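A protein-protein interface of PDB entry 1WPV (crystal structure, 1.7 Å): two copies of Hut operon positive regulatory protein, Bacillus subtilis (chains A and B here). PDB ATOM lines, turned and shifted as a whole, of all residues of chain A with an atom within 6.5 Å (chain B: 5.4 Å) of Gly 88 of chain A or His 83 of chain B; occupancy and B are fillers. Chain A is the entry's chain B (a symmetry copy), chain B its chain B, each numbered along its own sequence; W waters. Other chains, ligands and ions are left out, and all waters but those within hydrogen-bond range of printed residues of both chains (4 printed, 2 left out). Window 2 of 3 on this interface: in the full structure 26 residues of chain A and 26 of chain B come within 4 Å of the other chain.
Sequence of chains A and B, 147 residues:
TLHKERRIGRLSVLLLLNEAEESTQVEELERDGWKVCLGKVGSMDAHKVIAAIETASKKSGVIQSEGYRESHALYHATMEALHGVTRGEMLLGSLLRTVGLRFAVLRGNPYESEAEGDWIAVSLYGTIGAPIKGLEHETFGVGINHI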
ATOM      1  N   GLU A  80      31.292   3.206  -4.924  1.00  0.00           N
ATOM      2  CA  GLU A  80      31.838   4.532  -5.159  1.00  0.00           C
ATOM      3  C   GLU A  80      31.343   5.092  -6.488  1.00  0.00           C
ATOM      4  O   GLU A  80      30.996   6.267  -6.585  1.00  0.00           O
ATOM      5  CB  GLU A  80      33.373   4.492  -5.093  1.00  0.00           C
ATOM      6  CG  GLU A  80      33.884   4.227  -3.676  1.00  0.00           C
ATOM      7  CD  GLU A  80      35.350   4.586  -3.485  1.00  0.00           C
ATOM      8  OE1 GLU A  80      35.996   4.961  -4.484  1.00  0.00           O
ATOM      9  N   LEU A  82      28.549   4.323  -7.967  1.00  0.00           N
ATOM     10  CA  LEU A  82      27.130   4.645  -7.818  1.00  0.00           C
ATOM     11  C   LEU A  82      26.894   6.000  -7.166  1.00  0.00           C
ATOM     12  O   LEU A  82      25.853   6.621  -7.383  1.00  0.00           O
ATOM     13  CB  LEU A  82      26.409   3.543  -7.037  1.00  0.00           C
ATOM     14  CG  LEU A  82      26.133   2.293  -7.877  1.00  0.00           C
ATOM     15  CD1 LEU A  82      25.486   1.227  -7.009  1.00  0.00           C
ATOM     16  CD2 LEU A  82      25.235   2.648  -9.054  1.00  0.00           C
ATOM     17  N   HIS A  83      27.855   6.468  -6.371  1.00  0.00           N
ATOM     18  CA  HIS A  83      27.702   7.777  -5.740  1.00  0.00           C
ATOM     19  C   HIS A  83      27.589   8.887  -6.782  1.00  0.00           C
ATOM     20  O   HIS A  83      26.794   9.820  -6.622  1.00  0.00           O
ATOM     21  CB  HIS A  83      28.874   8.078  -4.806  1.00  0.00           C
ATOM     22  CG  HIS A  83      28.585   7.778  -3.371  1.00  0.00           C
ATOM     23  ND1 HIS A  83      29.275   6.825  -2.655  1.00  0.00           N
ATOM     24  CD2 HIS A  83      27.676   8.304  -2.517  1.00  0.00           C
ATOM     25  CE1 HIS A  83      28.804   6.776  -1.422  1.00  0.00           C
ATOM     26  NE2 HIS A  83      27.832   7.664  -1.312  1.00  0.00           N
ATOM     27  N   GLY A  84      28.378   8.800  -7.849  1.00  0.00           N
ATOM     28  CA  GLY A  84      28.297   9.825  -8.871  1.00  0.00           C
ATOM     29  C   GLY A  84      26.970   9.774  -9.605  1.00  0.00           C
ATOM     30  O   GLY A  84      26.439  10.798 -10.034  1.00  0.00           O
ATOM     31  N   THR A  86      23.969   8.470  -8.339  1.00  0.00           N
ATOM     32  CA  THR A  86      22.849   8.812  -7.462  1.00  0.00           C
ATOM     33  C   THR A  86      22.936  10.167  -6.764  1.00  0.00           C
ATOM     34  O   THR A  86      21.916  10.717  -6.345  1.00  0.00           O
ATOM     35  CB  THR A  86      22.656   7.721  -6.411  1.00  0.00           C
ATOM     36  OG1 THR A  86      23.871   7.562  -5.677  1.00  0.00           O
ATOM     37  CG2 THR A  86      22.287   6.411  -7.084  1.00  0.00           C
ATOM     38  N   ARG A  87      24.145  10.696  -6.617  1.00  0.00           N
ATOM     39  CA  ARG A  87      24.337  12.019  -6.011  1.00  0.00           C
ATOM     40  C   ARG A  87      23.599  12.311  -4.704  1.00  0.00           C
ATOM     41  O   ARG A  87      22.802  13.252  -4.632  1.00  0.00           O
ATOM     42  CB  ARG A  87      23.980  13.108  -7.037  1.00  0.00           C
ATOM     43  CG  ARG A  87      24.982  13.246  -8.184  1.00  0.00           C
ATOM     44  CD  ARG A  87      24.292  13.578  -9.494  1.00  0.00           C
ATOM     45  NE  ARG A  87      23.381  12.499  -9.881  1.00  0.00           N
ATOM     46  CZ  ARG A  87      22.086  12.665 -10.142  1.00  0.00           C
ATOM     47  NH1 ARG A  87      21.536  13.876 -10.075  1.00  0.00           N
ATOM     48  NH2 ARG A  87      21.330  11.607 -10.421  1.00  0.00           N
ATOM     49  N   GLY A  88      23.874  11.537  -3.662  1.00  0.00           N
ATOM     50  CA  GLY A  88      23.222  11.801  -2.390  1.00  0.00           C
ATOM     51  C   GLY A  88      22.523  10.620  -1.754  1.00  0.00           C
ATOM     52  O   GLY A  88      22.824  10.255  -0.621  1.00  0.00           O
ATOM     53  N   GLU A  89      21.579  10.031  -2.475  1.00  0.00           N
ATOM     54  CA  GLU A  89      20.837   8.876  -1.976  1.00  0.00           C
ATOM     55  C   GLU A  89      21.037   7.742  -2.972  1.00  0.00           C
ATOM     56  O   GLU A  89      20.628   7.860  -4.124  1.00  0.00           O
ATOM     57  CB  GLU A  89      19.346   9.205  -1.872  1.00  0.00           C
ATOM     58  CG  GLU A  89      18.989  10.299  -0.872  1.00  0.00           C
ATOM     59  CD  GLU A  89      19.382   9.948   0.548  1.00  0.00           C
ATOM     60  OE1 GLU A  89      19.008   8.851   1.026  1.00  0.00           O
ATOM     61  OE2 GLU A  89      20.063  10.775   1.190  1.00  0.00           O
ATOM     62  N   MET A  90      21.663   6.649  -2.538  1.00  0.00           N
ATOM     63  CA  MET A  90      21.915   5.528  -3.437  1.00  0.00           C
ATOM     64  C   MET A  90      20.632   4.734  -3.626  1.00  0.00           C
ATOM     65  O   MET A  90      20.561   3.535  -3.335  1.00  0.00           O
ATOM     66  CB  MET A  90      23.025   4.633  -2.878  1.00  0.00           C
ATOM     67  CG  MET A  90      23.822   3.935  -3.973  1.00  0.00           C
ATOM     68  SD  MET A  90      25.295   3.120  -3.333  1.00  0.00           S
ATOM     69  CE  MET A  90      26.401   4.552  -3.174  1.00  0.00           C
ATOM     70  N   LEU A  91      19.623   5.434  -4.128  1.00  0.00           N
ATOM     71  CA  LEU A  91      18.300   4.875  -4.360  1.00  0.00           C
ATOM     72  C   LEU A  91      17.814   5.228  -5.756  1.00  0.00           C
ATOM     73  O   LEU A  91      18.028   6.341  -6.236  1.00  0.00           O
ATOM     74  CB  LEU A  91      17.319   5.466  -3.357  1.00  0.00           C
ATOM     75  CG  LEU A  91      17.616   5.235  -1.880  1.00  0.00           C
ATOM     76  CD1 LEU A  91      16.726   6.157  -1.045  1.00  0.00           C
ATOM     77  CD2 LEU A  91      17.379   3.766  -1.542  1.00  0.00           C
ATOM     78  N   ARG A  97      12.906   6.934  -9.718  1.00  0.00           N
ATOM     79  CA  ARG A  97      13.812   7.160 -10.835  1.00  0.00           C
ATOM     80  C   ARG A  97      14.425   5.842 -11.300  1.00  0.00           C
ATOM     81  O   ARG A  97      14.486   4.866 -10.559  1.00  0.00           O
ATOM     82  CB  ARG A  97      14.900   8.198 -10.482  1.00  0.00           C
ATOM     83  CG  ARG A  97      15.812   7.851  -9.319  1.00  0.00           C
ATOM     84  CD  ARG A  97      16.827   8.971  -9.065  1.00  0.00           C
ATOM     85  NE  ARG A  97      17.661   8.663  -7.911  1.00  0.00           N
ATOM     86  CZ  ARG A  97      18.605   9.461  -7.420  1.00  0.00           C
ATOM     87  NH1 ARG A  97      18.853  10.635  -7.987  1.00  0.00           N
ATOM     88  NH2 ARG A  97      19.299   9.084  -6.354  1.00  0.00           N
ATOM     89  N   THR B  78      27.197  22.074  -9.645  1.00  0.00           N
ATOM     90  CA  THR B  78      28.526  21.895  -9.082  1.00  0.00           C
ATOM     91  C   THR B  78      28.460  20.920  -7.906  1.00  0.00           C
ATOM     92  O   THR B  78      29.314  20.044  -7.776  1.00  0.00           O
ATOM     93  CB  THR B  78      29.138  23.244  -8.603  1.00  0.00           C
ATOM     94  OG1 THR B  78      29.308  24.118  -9.727  1.00  0.00           O
ATOM     95  CG2 THR B  78      30.501  23.011  -7.957  1.00  0.00           C
ATOM     96  N   MET B  79      27.443  21.071  -7.059  1.00  0.00           N
ATOM     97  CA  MET B  79      27.277  20.179  -5.911  1.00  0.00           C
ATOM     98  C   MET B  79      27.120  18.739  -6.391  1.00  0.00           C
ATOM     99  O   MET B  79      27.729  17.819  -5.844  1.00  0.00           O
ATOM    100  CB  MET B  79      26.030  20.558  -5.101  1.00  0.00           C
ATOM    101  CG  MET B  79      26.110  21.882  -4.367  1.00  0.00           C
ATOM    102  SD  MET B  79      27.324  21.871  -3.031  1.00  0.00           S
ATOM    103  CE  MET B  79      28.688  22.538  -3.876  1.00  0.00           C
ATOM    104  N   GLU B  80      26.302  18.544  -7.418  1.00  0.00           N
ATOM    105  CA  GLU B  80      26.084  17.203  -7.933  1.00  0.00           C
ATOM    106  C   GLU B  80      27.388  16.606  -8.452  1.00  0.00           C
ATOM    107  O   GLU B  80      27.677  15.433  -8.223  1.00  0.00           O
ATOM    108  CB  GLU B  80      24.995  17.222  -9.017  1.00  0.00           C
ATOM    109  CG  GLU B  80      23.611  17.527  -8.441  1.00  0.00           C
ATOM    110  CD  GLU B  80      22.471  17.153  -9.376  1.00  0.00           C
ATOM    111  OE1 GLU B  80      22.761  16.735 -10.515  1.00  0.00           O
ATOM    112  N   ALA B  81      28.189  17.413  -9.140  1.00  0.00           N
ATOM    113  CA  ALA B  81      29.470  16.940  -9.650  1.00  0.00           C
ATOM    114  C   ALA B  81      30.387  16.562  -8.485  1.00  0.00           C
ATOM    115  O   ALA B  81      31.099  15.568  -8.549  1.00  0.00           O
ATOM    116  CB  ALA B  81      30.134  18.031 -10.500  1.00  0.00           C
ATOM    117  N   LEU B  82      30.381  17.365  -7.427  1.00  0.00           N
ATOM    118  CA  LEU B  82      31.230  17.070  -6.274  1.00  0.00           C
ATOM    119  C   LEU B  82      30.891  15.741  -5.612  1.00  0.00           C
ATOM    120  O   LEU B  82      31.747  15.128  -4.974  1.00  0.00           O
ATOM    121  CB  LEU B  82      31.161  18.208  -5.252  1.00  0.00           C
ATOM    122  CG  LEU B  82      31.984  19.433  -5.661  1.00  0.00           C
ATOM    123  CD1 LEU B  82      31.801  20.537  -4.633  1.00  0.00           C
ATOM    124  CD2 LEU B  82      33.453  19.052  -5.787  1.00  0.00           C
ATOM    125  N   HIS B  83      29.648  15.286  -5.763  1.00  0.00           N
ATOM    126  CA  HIS B  83      29.269  14.001  -5.179  1.00  0.00           C
ATOM    127  C   HIS B  83      30.095  12.859  -5.765  1.00  0.00           C
ATOM    128  O   HIS B  83      30.503  11.944  -5.041  1.00  0.00           O
ATOM    129  CB  HIS B  83      27.783  13.715  -5.397  1.00  0.00           C
ATOM    130  CG  HIS B  83      26.930  14.068  -4.222  1.00  0.00           C
ATOM    131  ND1 HIS B  83      25.950  15.033  -4.276  1.00  0.00           N
ATOM    132  CD2 HIS B  83      26.912  13.584  -2.958  1.00  0.00           C
ATOM    133  CE1 HIS B  83      25.365  15.131  -3.096  1.00  0.00           C
ATOM    134  NE2 HIS B  83      25.931  14.262  -2.277  1.00  0.00           N
ATOM    135  N   GLY B  84      30.344  12.898  -7.071  1.00  0.00           N
ATOM    136  CA  GLY B  84      31.135  11.841  -7.669  1.00  0.00           C
ATOM    137  C   GLY B  84      32.575  11.886  -7.194  1.00  0.00           C
ATOM    138  O   GLY B  84      33.235  10.856  -7.060  1.00  0.00           O
ATOM    139  N   VAL B  85      33.066  13.091  -6.938  1.00  0.00           N
ATOM    140  CA  VAL B  85      34.441  13.274  -6.490  1.00  0.00           C
ATOM    141  C   VAL B  85      34.628  12.867  -5.032  1.00  0.00           C
ATOM    142  O   VAL B  85      35.584  12.179  -4.690  1.00  0.00           O
ATOM    143  CB  VAL B  85      34.877  14.760  -6.654  1.00  0.00           C
ATOM    144  CG1 VAL B  85      36.184  15.031  -5.906  1.00  0.00           C
ATOM    145  CG2 VAL B  85      35.052  15.078  -8.134  1.00  0.00           C
ATOM    146  N   THR B  86      33.701  13.276  -4.175  1.00  0.00           N
ATOM    147  CA  THR B  86      33.811  12.981  -2.747  1.00  0.00           C
ATOM    148  C   THR B  86      33.219  11.649  -2.292  1.00  0.00           C
ATOM    149  O   THR B  86      33.595  11.129  -1.240  1.00  0.00           O
ATOM    150  CB  THR B  86      33.186  14.109  -1.930  1.00  0.00           C
ATOM    151  OG1 THR B  86      31.825  14.275  -2.330  1.00  0.00           O
ATOM    152  CG2 THR B  86      33.950  15.401  -2.159  1.00  0.00           C
ATOM    153  N   ARG B  87      32.283  11.108  -3.063  1.00  0.00           N
ATOM    154  CA  ARG B  87      31.689   9.803  -2.748  1.00  0.00           C
ATOM    155  C   ARG B  87      31.225   9.566  -1.311  1.00  0.00           C
ATOM    156  O   ARG B  87      31.699   8.640  -0.645  1.00  0.00           O
ATOM    157  CB  ARG B  87      32.668   8.685  -3.144  1.00  0.00           C
ATOM    158  CG  ARG B  87      32.828   8.494  -4.653  1.00  0.00           C
ATOM    159  CD  ARG B  87      34.254   8.128  -5.023  1.00  0.00           C
ATOM    160  NE  ARG B  87      35.172   9.207  -4.652  1.00  0.00           N
ATOM    161  CZ  ARG B  87      36.240   9.052  -3.873  1.00  0.00           C
ATOM    162  NH1 ARG B  87      36.546   7.852  -3.383  1.00  0.00           N
ATOM    163  NH2 ARG B  87      36.974  10.110  -3.543  1.00  0.00           N
ATOM    164  N   GLY B  88      30.285  10.371  -0.832  1.00  0.00           N
ATOM    165  CA  GLY B  88      29.789  10.159   0.518  1.00  0.00           C
ATOM    166  C   GLY B  88      29.813  11.372   1.423  1.00  0.00           C
ATOM    167  O   GLY B  88      28.782  11.771   1.957  1.00  0.00           O
ATOM    168  N   MET B  90      31.031  15.326   1.388  1.00  0.00           N
ATOM    169  CA  MET B  90      31.537  16.412   0.556  1.00  0.00           C
ATOM    170  C   MET B  90      32.558  17.218   1.344  1.00  0.00           C
ATOM    171  O   MET B  90      32.411  18.428   1.552  1.00  0.00           O
ATOM    172  CB  MET B  90      30.387  17.310   0.089  1.00  0.00           C
ATOM    173  CG  MET B  90      30.661  17.958  -1.262  1.00  0.00           C
ATOM    174  SD  MET B  90      29.203  18.772  -1.937  1.00  0.00           S
ATOM    175  CE  MET B  90      28.315  17.330  -2.594  1.00  0.00           C
HETATM  176  O   HOH W   1      31.423   8.557  -7.995  1.00  0.00           O
HETATM  177  O   HOH W   2      28.389  13.091  -9.414  1.00  0.00           O
HETATM  178  O   HOH W   3      32.167   6.066  -0.906  1.00  0.00           O
HETATM  179  O   HOH W   4      22.715  15.809  -5.241  1.00  0.00           O
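The backbone carbonyl oxygen (O) of Val 85 of chain B is in hydrogen-bond range of the guanidinium group (NH2) of Arg 87 of chain B, 2.7 Å away.
Gly 88 of chain A touches just one residue of chain B: His 83. Of the printed residues of chain A, His 83 of chain B touches Arg 87 (3.5 Å) and Gly 88 (3.7 Å). Of the printed residues of chain B, His 83 of chain A touches Arg 87 (3.5 Å) and Gly 88 (3.7 Å). Of the printed residues of chain B, Arg 87 of chain A touches Glu 80 and His 83. Of the printed residues of chain A, Gly 88 of chain B touches His 83. Printed residues of chain A within 4 Å of Arg 87 of chain B: Glu 80 and His 83. Thr 86 of chain B touches none of the printed residues of chain A. Thr 78 of chain B touches none of the printed residues of chain A. The nearest printed residue of chain B that does not touch Gly 88 of chain A is Gly 88 of chain B (6.7 Å). The nearest printed residue of chain B that does not touch Arg 87 of chain A is Ala 81 of chain B (5.3 Å).
OE1 of Glu 80 of chain B lies within salt-bridge range of NH1 of Arg 87 of chain A, at 3.1 Å. NH1 of Arg 87 of chain B is in salt-bridge range of OE1 of Glu 80 of chain A (3.1 Å).
Of the 11 printed residues of chain A, 5 touch a printed residue of chain B. Printed residues of chain A that touch a printed residue of chain B: Glu 80, His 83, Gly 84, Arg 87 and Gly 88. Hydrophobic or aromatic side chains of chain A that line the printed part of chain B: His 83. Along chain A the printed residues that touch a printed residue of chain B span positions 80 to 88. Among the printed residues, 7 pairs touch across the chains. Among the printed residues, Asp or Glu carboxylates within 4 Å of a Lys or Arg side-chain nitrogen of the other chain: Glu 80 of chain A with Arg 87 of chain B (3.1 Å) and Arg 87 of chain A with Glu 80 of chain B (3.1 Å).
Water W4 lies within hydrogen-bond range of O of Arg 87 of chain A (2.6 Å) and ND1 of His 83 of chain B (3.5 Å). Water W3 bridges the backbone carbonyl oxygen (O) of Arg 87 of chain B (2.6 Å) and a ring nitrogen (ND1) of His 83 of chain A (3.5 Å). Water W2 lies within hydrogen-bond range of the backbone carbonyl oxygen (O) of Glu 80 of chain B (2.7 Å), the backbone NH (N) of Gly 84 of chain B (3.1 Å) and the backbone carbonyl oxygen (O) of Gly 84 of chain A (3.1 Å). Water W1 lies within hydrogen-bond range of the backbone carbonyl oxygen (O) of Glu 80 of chain A (2.7 Å), the backbone NH (N) of Gly 84 of chain A (3.1 Å) and the backbone carbonyl oxygen (O) of Gly 84 of chain B (3.1 Å).
Glu 80 of chain A touches Arg 87 of chain B, and with the chains exchanged Arg 87 of chain A touches Glu 80 of chain B. His 83 of chain A touches Arg 87 of chain B, and with the chains exchanged Arg 87 of chain A touches His 83 of chain B. His 83 of chain A touches Gly 88 of chain B, and with the chains exchanged Gly 88 of chain A touches His 83 of chain B. Gly 84 of chain B touches its own counterpart, Gly 84 of chain A. 8 positions are printed for both chains. Of the 7 pairs that touch across the chains among the printed residues, 7 have their exchanged pair printed and touching as well.
Among the printed residues, pairs that only touch across the chains: Arg 87 of chain A with His 83 of chain B, His 83 of chain A with Arg 87 of chain B, His 83 of chain A with Gly 88 of chain B, Gly 88 of chain A with His 83 of chain B and Gly 84 of chain A with Gly 84 of chain B.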
